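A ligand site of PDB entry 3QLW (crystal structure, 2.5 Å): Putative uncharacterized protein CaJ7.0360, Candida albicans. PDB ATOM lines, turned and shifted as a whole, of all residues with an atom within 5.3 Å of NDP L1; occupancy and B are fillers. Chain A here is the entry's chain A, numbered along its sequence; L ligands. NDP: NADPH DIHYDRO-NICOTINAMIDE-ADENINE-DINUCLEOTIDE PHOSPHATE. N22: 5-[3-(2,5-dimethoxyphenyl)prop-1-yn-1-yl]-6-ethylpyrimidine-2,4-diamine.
An oxygen (O2D) of NDP L1 is in hydrogen-bond range of the backbone carbonyl oxygen (O) of Lys 24 (3.2 Å). The side-chain carboxylate (OE1) of Glu 120 sits at hydrogen-bond distance from a nitrogen (N6A) of NDP L1 (3.1 Å). The backbone NH of Gly 114 is in hydrogen-bond range of an oxygen (O2A) of NDP L1, 2.8 Å away. OG of Ser 78 sits at hydrogen-bond distance from O1X of NDP L1 (2.6 Å). An oxygen (O2X) of NDP L1 sits at hydrogen-bond distance from the backbone NH (N) of Arg 79 (2.8 Å). An oxygen (O7N) of NDP L1 lies within hydrogen-bond range of the backbone NH (N) of Ala 11 (3.0 Å). The guanidinium group of Arg 56 is in salt-bridge range of an oxygen (O1X) of NDP L1 (2.6 Å). O of Ile 112 is in hydrogen-bond range of N7 of N22 L2 (2.8 Å). N of Ala 115 sits at hydrogen-bond distance from O5D of NDP L1 (2.8 Å). NE of Arg 79 is in salt-bridge range of O2X of NDP L1. The backbone NH (N) of Glu 116 sits at hydrogen-bond distance from an oxygen (O2N) of NDP L1. A nitrogen (N7) of N22 L2 sits at hydrogen-bond distance from the side-chain hydroxyl (OH) of Tyr 118, 2.8 Å away. O2A of NDP L1 is in hydrogen-bond range of OG1 of Thr 58, 2.5 Å away. The backbone NH of Val 10 lies close to a nitrogen (N2) of N22 L2 (3.3 Å). N of Ile 117 lies close to O1A of NDP L1, at 3.5 Å. The backbone NH (N) of Ser 78 is in hydrogen-bond range of a nitrogen (N3A) of NDP L1. A nitrogen (N7) of N22 L2 lies within hydrogen-bond range of the backbone carbonyl oxygen (O) of Ile 9, 2.9 Å away. The backbone NH (N) of Thr 58 sits at hydrogen-bond distance from an oxygen (O2A) of NDP L1 (3.2 Å). The backbone carbonyl oxygen (O) of Ala 11 lies within hydrogen-bond range of a nitrogen (N7N) of NDP L1, 2.8 Å away.
The side-chain hydroxyl of Ser 78 sits close to the backbone NH of Ser 80 (3.2 Å). The backbone carbonyl oxygen (O) of Ile 112 is in hydrogen-bond range of the side-chain hydroxyl (OH) of Tyr 118. O of Leu 77 is in hydrogen-bond range of N of Arg 56 (3.0 Å). OH of Tyr 118 lies within hydrogen-bond range of N of Gly 113 (3.5 Å). N of Ile 19 sits at hydrogen-bond distance from O of Thr 147 (2.9 Å). The backbone NH (N) of Gly 55 is in hydrogen-bond range of the backbone carbonyl oxygen (O) of Gly 113. O of Met 54 sits at hydrogen-bond distance from N of Leu 77, 2.8 Å away. The backbone carbonyl oxygen (O) of Gly 20 is in hydrogen-bond range of the backbone NH (N) of Thr 147 (3.2 Å).
N1A of NDP L1 lies close to O of Ser 94 (2.9 Å). Residues that only touch NDP L1: Ile 112 (3.1 Å), Gly 23 (3.3 Å), Leu 77 (3.3 Å), Val 10 (3.4 Å), Lys 57 (3.5 Å), Tyr 118 (3.5 Å), Ile 19 (3.5 Å), Met 25 (3.5 Å), Gly 55 (3.6 Å), Gly 113 (3.7 Å) and Gly 20 (3.9 Å). Hydrophobic or aromatic side chains that line NDP L1: Val 10, Ile 19, Met 25, Leu 77, Ala 115 and Ile 117. Within 4 Å of NDP L1: Val 10, Ala 11, Ile 19, Gly 20, Gly 23, Lys 24, Met 25, Gly 55, Arg 56, Lys 57, Thr 58, Leu 77, Ser 78, Arg 79, Ser 94, Ile 112, Gly 113, Gly 114, Ala 115, Glu 116, Ile 117, Tyr 118 and Glu 120. The nearest printed residue that does not touch NDP L1 is Trp 27 (4.1 Å).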
ATOM      1  N   ILE A   9      -1.126  -0.206  -2.104  1.00  0.00           N
ATOM      2  CA  ILE A   9      -0.492  -0.982  -1.036  1.00  0.00           C
ATOM      3  C   ILE A   9      -1.217  -0.686   0.279  1.00  0.00           C
ATOM      4  O   ILE A   9      -1.418   0.482   0.634  1.00  0.00           O
ATOM      5  CB  ILE A   9       1.043  -0.712  -0.972  1.00  0.00           C
ATOM      6  CG1 ILE A   9       1.711  -1.550   0.134  1.00  0.00           C
ATOM      7  CG2 ILE A   9       1.352   0.786  -0.840  1.00  0.00           C
ATOM      8  CD1 ILE A   9       3.199  -1.747  -0.051  1.00  0.00           C
ATOM      9  N   VAL A  10      -1.612  -1.745   0.987  1.00  0.00           N
ATOM     10  CA  VAL A  10      -2.393  -1.650   2.225  1.00  0.00           C
ATOM     11  C   VAL A  10      -2.271  -2.919   3.069  1.00  0.00           C
ATOM     12  O   VAL A  10      -2.042  -4.010   2.536  1.00  0.00           O
ATOM     13  CB  VAL A  10      -3.913  -1.340   1.931  1.00  0.00           C
ATOM     14  CG1 VAL A  10      -4.566  -2.454   1.100  1.00  0.00           C
ATOM     15  CG2 VAL A  10      -4.683  -1.082   3.218  1.00  0.00           C
ATOM     16  N   ALA A  11      -2.411  -2.769   4.385  1.00  0.00           N
ATOM     17  CA  ALA A  11      -2.511  -3.890   5.311  1.00  0.00           C
ATOM     18  C   ALA A  11      -3.875  -3.886   6.003  1.00  0.00           C
ATOM     19  O   ALA A  11      -4.269  -2.888   6.609  1.00  0.00           O
ATOM     20  CB  ALA A  11      -1.376  -3.846   6.330  1.00  0.00           C
ATOM     21  N   ALA A  12      -4.590  -4.995   5.887  1.00  0.00           N
ATOM     22  CA  ALA A  12      -5.972  -5.077   6.350  1.00  0.00           C
ATOM     23  C   ALA A  12      -6.259  -6.388   7.081  1.00  0.00           C
ATOM     24  O   ALA A  12      -5.652  -7.419   6.774  1.00  0.00           O
ATOM     25  CB  ALA A  12      -6.939  -4.902   5.189  1.00  0.00           C
ATOM     26  N   ILE A  19      -9.032  -1.408   8.537  1.00  0.00           N
ATOM     27  CA  ILE A  19      -7.716  -0.786   8.376  1.00  0.00           C
ATOM     28  C   ILE A  19      -7.384   0.248   9.445  1.00  0.00           C
ATOM     29  O   ILE A  19      -6.215   0.618   9.619  1.00  0.00           O
ATOM     30  CB  ILE A  19      -7.540  -0.155   6.971  1.00  0.00           C
ATOM     31  CG1 ILE A  19      -8.659   0.863   6.682  1.00  0.00           C
ATOM     32  CG2 ILE A  19      -7.479  -1.235   5.891  1.00  0.00           C
ATOM     33  CD1 ILE A  19      -8.344   1.840   5.555  1.00  0.00           C
ATOM     34  N   GLY A  20      -8.397   0.716  10.170  1.00  0.00           N
ATOM     35  CA  GLY A  20      -8.181   1.712  11.205  1.00  0.00           C
ATOM     36  C   GLY A  20      -9.297   1.876  12.218  1.00  0.00           C
ATOM     37  O   GLY A  20     -10.415   1.422  12.003  1.00  0.00           O
ATOM     38  N   TYR A  21      -8.961   2.522  13.330  1.00  0.00           N
ATOM     39  CA  TYR A  21      -9.941   2.882  14.360  1.00  0.00           C
ATOM     40  C   TYR A  21      -9.627   4.276  14.882  1.00  0.00           C
ATOM     41  O   TYR A  21      -8.515   4.542  15.339  1.00  0.00           O
ATOM     42  CB  TYR A  21      -9.952   1.863  15.500  1.00  0.00           C
ATOM     43  CG  TYR A  21     -10.892   2.222  16.637  1.00  0.00           C
ATOM     44  CD1 TYR A  21     -12.276   2.088  16.497  1.00  0.00           C
ATOM     45  CD2 TYR A  21     -10.393   2.679  17.856  1.00  0.00           C
ATOM     46  CE1 TYR A  21     -13.139   2.419  17.540  1.00  0.00           C
ATOM     47  CE2 TYR A  21     -11.252   3.008  18.912  1.00  0.00           C
ATOM     48  CZ  TYR A  21     -12.616   2.870  18.743  1.00  0.00           C
ATOM     49  OH  TYR A  21     -13.473   3.189  19.782  1.00  0.00           O
ATOM     50  N   LYS A  22     -10.626   5.163  14.801  1.00  0.00           N
ATOM     51  CA  LYS A  22     -10.524   6.561  15.247  1.00  0.00           C
ATOM     52  C   LYS A  22      -9.249   7.244  14.739  1.00  0.00           C
ATOM     53  O   LYS A  22      -8.494   7.846  15.519  1.00  0.00           O
ATOM     54  CB  LYS A  22     -10.633   6.668  16.774  1.00  0.00           C
ATOM     55  CG  LYS A  22     -11.973   6.212  17.369  1.00  0.00           C
ATOM     56  CD  LYS A  22     -13.146   7.066  16.902  1.00  0.00           C
ATOM     57  CE  LYS A  22     -14.396   6.800  17.742  1.00  0.00           C
ATOM     58  NZ  LYS A  22     -14.302   7.382  19.113  1.00  0.00           N
ATOM     59  N   GLY A  23      -9.019   7.164  13.425  1.00  0.00           N
ATOM     60  CA  GLY A  23      -7.869   7.804  12.793  1.00  0.00           C
ATOM     61  C   GLY A  23      -6.530   7.114  13.032  1.00  0.00           C
ATOM     62  O   GLY A  23      -5.503   7.583  12.543  1.00  0.00           O
ATOM     63  N   LYS A  24      -6.546   6.017  13.780  1.00  0.00           N
ATOM     64  CA  LYS A  24      -5.318   5.299  14.128  1.00  0.00           C
ATOM     65  C   LYS A  24      -5.213   3.951  13.442  1.00  0.00           C
ATOM     66  O   LYS A  24      -6.207   3.401  12.969  1.00  0.00           O
ATOM     67  CB  LYS A  24      -5.237   5.082  15.644  1.00  0.00           C
ATOM     68  CG  LYS A  24      -4.896   6.317  16.463  1.00  0.00           C
ATOM     69  CD  LYS A  24      -4.913   5.990  17.941  1.00  0.00           C
ATOM     70  CE  LYS A  24      -6.328   5.946  18.506  1.00  0.00           C
ATOM     71  NZ  LYS A  24      -6.882   7.310  18.724  1.00  0.00           N
ATOM     72  N   MET A  25      -3.994   3.412  13.415  1.00  0.00           N
ATOM     73  CA  MET A  25      -3.747   2.062  12.959  1.00  0.00           C
ATOM     74  C   MET A  25      -3.893   1.108  14.144  1.00  0.00           C
ATOM     75  O   MET A  25      -3.336   1.365  15.216  1.00  0.00           O
ATOM     76  CB  MET A  25      -2.336   1.967  12.378  1.00  0.00           C
ATOM     77  CG  MET A  25      -2.205   1.016  11.220  1.00  0.00           C
ATOM     78  SD  MET A  25      -0.944   1.572  10.070  1.00  0.00           S
ATOM     79  CE  MET A  25      -1.762   2.954   9.281  1.00  0.00           C
ATOM     80  N   TRP A  27      -2.717  -1.742  14.736  1.00  0.00           N
ATOM     81  CA  TRP A  27      -1.600  -2.664  14.913  1.00  0.00           C
ATOM     82  C   TRP A  27      -0.258  -1.995  14.637  1.00  0.00           C
ATOM     83  O   TRP A  27      -0.190  -0.991  13.922  1.00  0.00           O
ATOM     84  CB  TRP A  27      -1.766  -3.888  14.010  1.00  0.00           C
ATOM     85  CG  TRP A  27      -2.196  -3.556  12.609  1.00  0.00           C
ATOM     86  CD1 TRP A  27      -1.428  -3.006  11.618  1.00  0.00           C
ATOM     87  CD2 TRP A  27      -3.502  -3.740  12.045  1.00  0.00           C
ATOM     88  NE1 TRP A  27      -2.174  -2.834  10.476  1.00  0.00           N
ATOM     89  CE2 TRP A  27      -3.444  -3.283  10.705  1.00  0.00           C
ATOM     90  CE3 TRP A  27      -4.711  -4.265  12.528  1.00  0.00           C
ATOM     91  CZ2 TRP A  27      -4.554  -3.321   9.846  1.00  0.00           C
ATOM     92  CZ3 TRP A  27      -5.817  -4.305  11.682  1.00  0.00           C
ATOM     93  CH2 TRP A  27      -5.729  -3.836  10.348  1.00  0.00           C
ATOM     94  N   MET A  54      -1.189   9.890  -1.204  1.00  0.00           N
ATOM     95  CA  MET A  54      -1.967   9.753   0.016  1.00  0.00           C
ATOM     96  C   MET A  54      -2.991  10.877   0.214  1.00  0.00           C
ATOM     97  O   MET A  54      -2.914  11.913  -0.438  1.00  0.00           O
ATOM     98  CB  MET A  54      -1.039   9.669   1.238  1.00  0.00           C
ATOM     99  CG  MET A  54      -0.404  10.993   1.641  1.00  0.00           C
ATOM    100  SD  MET A  54       1.040  10.768   2.685  1.00  0.00           S
ATOM    101  CE  MET A  54       2.315  10.541   1.444  1.00  0.00           C
ATOM    102  N   GLY A  55      -3.935  10.649   1.126  1.00  0.00           N
ATOM    103  CA  GLY A  55      -4.878  11.688   1.539  1.00  0.00           C
ATOM    104  C   GLY A  55      -4.204  12.629   2.515  1.00  0.00           C
ATOM    105  O   GLY A  55      -3.204  12.276   3.147  1.00  0.00           O
ATOM    106  N   ARG A  56      -4.767  13.829   2.639  1.00  0.00           N
ATOM    107  CA  ARG A  56      -4.258  14.832   3.578  1.00  0.00           C
ATOM    108  C   ARG A  56      -4.210  14.314   5.007  1.00  0.00           C
ATOM    109  O   ARG A  56      -3.254  14.577   5.740  1.00  0.00           O
ATOM    110  CB  ARG A  56      -5.093  16.120   3.494  1.00  0.00           C
ATOM    111  CG  ARG A  56      -4.695  17.213   4.489  1.00  0.00           C
ATOM    112  CD  ARG A  56      -5.652  18.397   4.476  1.00  0.00           C
ATOM    113  NE  ARG A  56      -7.057  17.987   4.501  1.00  0.00           N
ATOM    114  CZ  ARG A  56      -7.766  17.743   5.601  1.00  0.00           C
ATOM    115  NH1 ARG A  56      -7.218  17.849   6.802  1.00  0.00           N
ATOM    116  NH2 ARG A  56      -9.034  17.367   5.491  1.00  0.00           N
ATOM    117  N   LYS A  57      -5.245  13.559   5.402  1.00  0.00           N
ATOM    118  CA  LYS A  57      -5.342  13.016   6.764  1.00  0.00           C
ATOM    119  C   LYS A  57      -4.252  12.008   7.103  1.00  0.00           C
ATOM    120  O   LYS A  57      -3.710  12.026   8.214  1.00  0.00           O
ATOM    121  CB  LYS A  57      -6.733  12.417   7.009  1.00  0.00           C
ATOM    122  CG  LYS A  57      -7.810  13.454   7.309  1.00  0.00           C
ATOM    123  CD  LYS A  57      -9.185  12.812   7.374  1.00  0.00           C
ATOM    124  CE  LYS A  57     -10.276  13.865   7.515  1.00  0.00           C
ATOM    125  NZ  LYS A  57     -11.617  13.293   7.268  1.00  0.00           N
ATOM    126  N   THR A  58      -3.920  11.126   6.151  1.00  0.00           N
ATOM    127  CA  THR A  58      -2.831  10.168   6.325  1.00  0.00           C
ATOM    128  C   THR A  58      -1.490  10.891   6.454  1.00  0.00           C
ATOM    129  O   THR A  58      -0.673  10.535   7.302  1.00  0.00           O
ATOM    130  CB  THR A  58      -2.801   9.131   5.172  1.00  0.00           C
ATOM    131  OG1 THR A  58      -4.033   8.396   5.162  1.00  0.00           O
ATOM    132  CG2 THR A  58      -1.641   8.152   5.339  1.00  0.00           C
ATOM    133  N   LEU A  77      -3.139  14.533  -1.295  1.00  0.00           N
ATOM    134  CA  LEU A  77      -4.405  14.825  -1.949  1.00  0.00           C
ATOM    135  C   LEU A  77      -5.377  15.559  -1.047  1.00  0.00           C
ATOM    136  O   LEU A  77      -5.617  15.164   0.095  1.00  0.00           O
ATOM    137  CB  LEU A  77      -5.049  13.546  -2.516  1.00  0.00           C
ATOM    138  CG  LEU A  77      -4.399  12.879  -3.733  1.00  0.00           C
ATOM    139  CD1 LEU A  77      -5.296  11.778  -4.270  1.00  0.00           C
ATOM    140  CD2 LEU A  77      -4.078  13.874  -4.836  1.00  0.00           C
ATOM    141  N   SER A  78      -5.913  16.657  -1.575  1.00  0.00           N
ATOM    142  CA  SER A  78      -6.966  17.418  -0.936  1.00  0.00           C
ATOM    143  C   SER A  78      -7.799  18.054  -2.034  1.00  0.00           C
ATOM    144  O   SER A  78      -7.308  18.282  -3.142  1.00  0.00           O
ATOM    145  CB  SER A  78      -6.385  18.490  -0.018  1.00  0.00           C
ATOM    146  OG  SER A  78      -7.397  19.359   0.473  1.00  0.00           O
ATOM    147  N   ARG A  79      -9.071  18.319  -1.732  1.00  0.00           N
ATOM    148  CA  ARG A  79      -9.956  18.939  -2.699  1.00  0.00           C
ATOM    149  C   ARG A  79      -9.741  20.447  -2.776  1.00  0.00           C
ATOM    150  O   ARG A  79     -10.256  21.118  -3.661  1.00  0.00           O
ATOM    151  CB  ARG A  79     -11.421  18.589  -2.391  1.00  0.00           C
ATOM    152  CG  ARG A  79     -11.802  17.192  -2.860  1.00  0.00           C
ATOM    153  CD  ARG A  79     -13.213  16.838  -2.442  1.00  0.00           C
ATOM    154  NE  ARG A  79     -13.255  16.255  -1.100  1.00  0.00           N
ATOM    155  CZ  ARG A  79     -13.207  14.936  -0.855  1.00  0.00           C
ATOM    156  NH1 ARG A  79     -13.111  14.070  -1.857  1.00  0.00           N
ATOM    157  NH2 ARG A  79     -13.253  14.501   0.394  1.00  0.00           N
ATOM    158  N   SER A  80      -8.972  20.959  -1.818  1.00  0.00           N
ATOM    159  CA  SER A  80      -8.603  22.378  -1.775  1.00  0.00           C
ATOM    160  C   SER A  80      -7.344  22.680  -2.589  1.00  0.00           C
ATOM    161  O   SER A  80      -7.107  23.823  -2.966  1.00  0.00           O
ATOM    162  CB  SER A  80      -8.372  22.802  -0.329  1.00  0.00           C
ATOM    163  OG  SER A  80      -9.552  22.629   0.441  1.00  0.00           O
ATOM    164  N   ALA A  93      -1.939  18.077  -4.757  1.00  0.00           N
ATOM    165  CA  ALA A  93      -2.774  17.820  -5.943  1.00  0.00           C
ATOM    166  C   ALA A  93      -4.258  17.661  -5.640  1.00  0.00           C
ATOM    167  O   ALA A  93      -4.649  17.353  -4.513  1.00  0.00           O
ATOM    168  CB  ALA A  93      -2.261  16.596  -6.700  1.00  0.00           C
ATOM    169  N   SER A  94      -5.080  17.888  -6.669  1.00  0.00           N
ATOM    170  CA  SER A  94      -6.537  17.748  -6.593  1.00  0.00           C
ATOM    171  C   SER A  94      -6.970  16.316  -6.920  1.00  0.00           C
ATOM    172  O   SER A  94      -8.032  15.878  -6.497  1.00  0.00           O
ATOM    173  CB  SER A  94      -7.217  18.695  -7.577  1.00  0.00           C
ATOM    174  OG  SER A  94      -6.723  20.021  -7.450  1.00  0.00           O
ATOM    175  N   SER A  95      -6.139  15.614  -7.690  1.00  0.00           N
ATOM    176  CA  SER A  95      -6.445  14.256  -8.141  1.00  0.00           C
ATOM    177  C   SER A  95      -5.162  13.519  -8.522  1.00  0.00           C
ATOM    178  O   SER A  95      -4.108  14.141  -8.682  1.00  0.00           O
ATOM    179  CB  SER A  95      -7.387  14.306  -9.356  1.00  0.00           C
ATOM    180  OG  SER A  95      -6.741  14.907 -10.477  1.00  0.00           O
ATOM    181  N   ILE A 112      -1.044   4.877  -0.786  1.00  0.00           N
ATOM    182  CA  ILE A 112      -0.720   4.398   0.551  1.00  0.00           C
ATOM    183  C   ILE A 112      -1.790   4.725   1.614  1.00  0.00           C
ATOM    184  O   ILE A 112      -1.592   4.430   2.793  1.00  0.00           O
ATOM    185  CB  ILE A 112       0.691   4.862   1.013  1.00  0.00           C
ATOM    186  CG1 ILE A 112       0.740   6.372   1.277  1.00  0.00           C
ATOM    187  CG2 ILE A 112       1.755   4.442  -0.011  1.00  0.00           C
ATOM    188  CD1 ILE A 112       1.930   6.812   2.126  1.00  0.00           C
ATOM    189  N   GLY A 113      -2.911   5.309   1.188  1.00  0.00           N
ATOM    190  CA  GLY A 113      -4.022   5.579   2.096  1.00  0.00           C
ATOM    191  C   GLY A 113      -4.528   7.011   2.095  1.00  0.00           C
ATOM    192  O   GLY A 113      -4.037   7.851   1.346  1.00  0.00           O
ATOM    193  N   GLY A 114      -5.537   7.301   2.932  1.00  0.00           N
ATOM    194  CA  GLY A 114      -6.197   6.294   3.750  1.00  0.00           C
ATOM    195  C   GLY A 114      -7.468   5.766   3.128  1.00  0.00           C
ATOM    196  O   GLY A 114      -7.526   5.530   1.913  1.00  0.00           O
ATOM    197  N   ALA A 115      -8.491   5.599   3.966  1.00  0.00           N
ATOM    198  CA  ALA A 115      -9.752   4.943   3.599  1.00  0.00           C
ATOM    199  C   ALA A 115     -10.476   5.581   2.417  1.00  0.00           C
ATOM    200  O   ALA A 115     -10.865   4.874   1.472  1.00  0.00           O
ATOM    201  CB  ALA A 115     -10.664   4.861   4.800  1.00  0.00           C
ATOM    202  N   GLU A 116     -10.675   6.894   2.462  1.00  0.00           N
ATOM    203  CA  GLU A 116     -11.399   7.600   1.391  1.00  0.00           C
ATOM    204  C   GLU A 116     -10.622   7.539   0.076  1.00  0.00           C
ATOM    205  O   GLU A 116     -11.216   7.427  -0.988  1.00  0.00           O
ATOM    206  CB  GLU A 116     -11.695   9.046   1.790  1.00  0.00           C
ATOM    207  CG  GLU A 116     -12.755   9.720   0.917  1.00  0.00           C
ATOM    208  CD  GLU A 116     -12.962  11.187   1.242  1.00  0.00           C
ATOM    209  OE1 GLU A 116     -12.258  11.718   2.127  1.00  0.00           O
ATOM    210  OE2 GLU A 116     -13.845  11.828   0.619  1.00  0.00           O
ATOM    211  N   ILE A 117      -9.298   7.611   0.164  1.00  0.00           N
ATOM    212  CA  ILE A 117      -8.419   7.486  -0.993  1.00  0.00           C
ATOM    213  C   ILE A 117      -8.502   6.084  -1.606  1.00  0.00           C
ATOM    214  O   ILE A 117      -8.696   5.959  -2.815  1.00  0.00           O
ATOM    215  CB  ILE A 117      -6.939   7.835  -0.621  1.00  0.00           C
ATOM    216  CG1 ILE A 117      -6.841   9.262  -0.077  1.00  0.00           C
ATOM    217  CG2 ILE A 117      -6.001   7.636  -1.813  1.00  0.00           C
ATOM    218  CD1 ILE A 117      -7.327  10.360  -1.026  1.00  0.00           C
ATOM    219  N   TYR A 118      -8.362   5.064  -0.763  1.00  0.00           N
ATOM    220  CA  TYR A 118      -8.431   3.655  -1.200  1.00  0.00           C
ATOM    221  C   TYR A 118      -9.760   3.342  -1.878  1.00  0.00           C
ATOM    222  O   TYR A 118      -9.795   2.881  -3.012  1.00  0.00           O
ATOM    223  CB  TYR A 118      -8.258   2.704  -0.014  1.00  0.00           C
ATOM    224  CG  TYR A 118      -6.863   2.536   0.547  1.00  0.00           C
ATOM    225  CD1 TYR A 118      -5.750   2.387  -0.303  1.00  0.00           C
ATOM    226  CD2 TYR A 118      -6.655   2.467   1.921  1.00  0.00           C
ATOM    227  CE1 TYR A 118      -4.474   2.209   0.231  1.00  0.00           C
ATOM    228  CE2 TYR A 118      -5.393   2.291   2.453  1.00  0.00           C
ATOM    229  CZ  TYR A 118      -4.305   2.163   1.601  1.00  0.00           C
ATOM    230  OH  TYR A 118      -3.061   1.987   2.154  1.00  0.00           O
ATOM    231  N   GLU A 120     -11.981   5.054  -3.204  1.00  0.00           N
ATOM    232  CA  GLU A 120     -12.247   5.751  -4.463  1.00  0.00           C
ATOM    233  C   GLU A 120     -11.344   5.292  -5.603  1.00  0.00           C
ATOM    234  O   GLU A 120     -11.822   5.046  -6.710  1.00  0.00           O
ATOM    235  CB  GLU A 120     -12.140   7.274  -4.270  1.00  0.00           C
ATOM    236  CG  GLU A 120     -13.326   7.863  -3.522  1.00  0.00           C
ATOM    237  CD  GLU A 120     -13.346   9.372  -3.538  1.00  0.00           C
ATOM    238  OE1 GLU A 120     -12.309   9.987  -3.213  1.00  0.00           O
ATOM    239  OE2 GLU A 120     -14.420   9.937  -3.870  1.00  0.00           O
ATOM    240  N   THR A 147     -13.166   1.717  10.471  1.00  0.00           N
ATOM    241  CA  THR A 147     -12.720   2.104   9.132  1.00  0.00           C
ATOM    242  C   THR A 147     -12.384   0.866   8.299  1.00  0.00           C
ATOM    243  O   THR A 147     -11.541   0.055   8.693  1.00  0.00           O
ATOM    244  CB  THR A 147     -11.504   3.032   9.205  1.00  0.00           C
ATOM    245  OG1 THR A 147     -11.700   4.001  10.245  1.00  0.00           O
ATOM    246  CG2 THR A 147     -11.300   3.754   7.890  1.00  0.00           C
HETATM  247  PA  NDP L   1      -7.438   9.940   4.076  1.00  0.00           P
HETATM  248  O1A NDP L   1      -7.998   9.104   2.994  1.00  0.00           O
HETATM  249  O2A NDP L   1      -6.002   9.658   4.290  1.00  0.00           O
HETATM  250  O5B NDP L   1      -7.670  11.503   3.772  1.00  0.00           O
HETATM  251  C5B NDP L   1      -8.944  11.979   3.428  1.00  0.00           C
HETATM  252  C4B NDP L   1      -8.752  13.318   2.720  1.00  0.00           C
HETATM  253  O4B NDP L   1      -8.210  13.122   1.427  1.00  0.00           O
HETATM  254  C3B NDP L   1     -10.049  14.074   2.517  1.00  0.00           C
HETATM  255  O3B NDP L   1     -10.390  14.826   3.654  1.00  0.00           O
HETATM  256  C2B NDP L   1      -9.719  14.934   1.318  1.00  0.00           C
HETATM  257  O2B NDP L   1      -8.994  16.082   1.712  1.00  0.00           O
HETATM  258  C1B NDP L   1      -8.742  14.078   0.530  1.00  0.00           C
HETATM  259  N9A NDP L   1      -9.393  13.391  -0.607  1.00  0.00           N
HETATM  260  C8A NDP L   1     -10.254  12.320  -0.550  1.00  0.00           C
HETATM  261  N7A NDP L   1     -10.605  11.977  -1.810  1.00  0.00           N
HETATM  262  C5A NDP L   1      -9.978  12.824  -2.668  1.00  0.00           C
HETATM  263  C6A NDP L   1      -9.983  12.921  -4.064  1.00  0.00           C
HETATM  264  N6A NDP L   1     -10.712  12.079  -4.790  1.00  0.00           N
HETATM  265  N1A NDP L   1      -9.226  13.893  -4.672  1.00  0.00           N
HETATM  266  C2A NDP L   1      -8.469  14.767  -3.905  1.00  0.00           C
HETATM  267  N3A NDP L   1      -8.469  14.667  -2.530  1.00  0.00           N
HETATM  268  C4A NDP L   1      -9.210  13.709  -1.918  1.00  0.00           C
HETATM  269  O3  NDP L   1      -8.253   9.729   5.448  1.00  0.00           O
HETATM  270  PN  NDP L   1      -9.281   8.594   5.918  1.00  0.00           P
HETATM  271  O1N NDP L   1      -9.885   9.030   7.199  1.00  0.00           O
HETATM  272  O2N NDP L   1     -10.152   8.254   4.775  1.00  0.00           O
HETATM  273  O5D NDP L   1      -8.322   7.340   6.199  1.00  0.00           O
HETATM  274  C5D NDP L   1      -7.420   7.365   7.290  1.00  0.00           C
HETATM  275  C4D NDP L   1      -7.502   6.041   8.044  1.00  0.00           C
HETATM  276  O4D NDP L   1      -6.932   5.011   7.263  1.00  0.00           O
HETATM  277  C3D NDP L   1      -6.736   6.086   9.354  1.00  0.00           C
HETATM  278  O3D NDP L   1      -7.497   5.446  10.350  1.00  0.00           O
HETATM  279  C2D NDP L   1      -5.482   5.285   9.086  1.00  0.00           C
HETATM  280  O2D NDP L   1      -5.053   4.591  10.241  1.00  0.00           O
HETATM  281  C1D NDP L   1      -5.931   4.322   8.003  1.00  0.00           C
HETATM  282  N1N NDP L   1      -4.833   3.866   7.128  1.00  0.00           N
HETATM  283  C2N NDP L   1      -4.559   2.530   7.091  1.00  0.00           C
HETATM  284  C3N NDP L   1      -3.537   2.029   6.281  1.00  0.00           C
HETATM  285  C7N NDP L   1      -3.190   0.566   6.332  1.00  0.00           C
HETATM  286  O7N NDP L   1      -2.341   0.023   5.348  1.00  0.00           O
HETATM  287  N7N NDP L   1      -3.698  -0.189   7.309  1.00  0.00           N
HETATM  288  C4N NDP L   1      -2.795   2.914   5.503  1.00  0.00           C
HETATM  289  C5N NDP L   1      -3.091   4.285   5.531  1.00  0.00           C
HETATM  290  C6N NDP L   1      -4.113   4.748   6.350  1.00  0.00           C
HETATM  291  P2B NDP L   1      -9.703  17.489   2.030  1.00  0.00           P
HETATM  292  O1X NDP L   1      -8.638  18.436   2.541  1.00  0.00           O
HETATM  293  O2X NDP L   1     -10.320  18.034   0.771  1.00  0.00           O
HETATM  294  O3X NDP L   1     -10.735  17.303   3.119  1.00  0.00           O
HETATM  295  C8  N22 L   2       1.693   0.511   8.060  1.00  0.00           C
HETATM  296  C7  N22 L   2       2.546   0.735   6.822  1.00  0.00           C
HETATM  297  C5  N22 L   2       1.734   0.440   5.545  1.00  0.00           C
HETATM  298  N4  N22 L   2       1.750  -0.897   5.098  1.00  0.00           N
HETATM  299  C3  N22 L   2       1.050  -1.266   3.950  1.00  0.00           C
HETATM  300  N8  N22 L   2       1.069  -2.523   3.516  1.00  0.00           N
HETATM  301  N2  N22 L   2       0.326  -0.307   3.244  1.00  0.00           N
HETATM  302  C1  N22 L   2       0.294   1.015   3.686  1.00  0.00           C
HETATM  303  N7  N22 L   2      -0.407   1.899   2.989  1.00  0.00           N
HETATM  304  C6  N22 L   2       0.994   1.384   4.834  1.00  0.00           C
HETATM  305  C9  N22 L   2       0.946   2.759   5.246  1.00  0.00           C
HETATM  306  C10 N22 L   2       0.875   3.937   5.570  1.00  0.00           C
HETATM  307  C11 N22 L   2       0.805   5.351   5.982  1.00  0.00           C
HETATM  308  C13 N22 L   2       1.737   5.588   7.175  1.00  0.00           C
HETATM  309  C18 N22 L   2       3.083   5.300   6.972  1.00  0.00           C
HETATM  310  C17 N22 L   2       4.021   5.471   7.985  1.00  0.00           C
HETATM  311  O2  N22 L   2       5.335   5.186   7.755  1.00  0.00           O
HETATM  312  C4  N22 L   2       5.606   3.764   7.743  1.00  0.00           C
HETATM  313  C16 N22 L   2       3.606   5.956   9.231  1.00  0.00           C
HETATM  314  C15 N22 L   2       2.251   6.243   9.444  1.00  0.00           C
HETATM  315  C14 N22 L   2       1.319   6.060   8.428  1.00  0.00           C
HETATM  316  O10 N22 L   2      -0.009   6.353   8.618  1.00  0.00           O
HETATM  317  C2  N22 L   2      -0.449   6.449   9.986  1.00  0.00           C
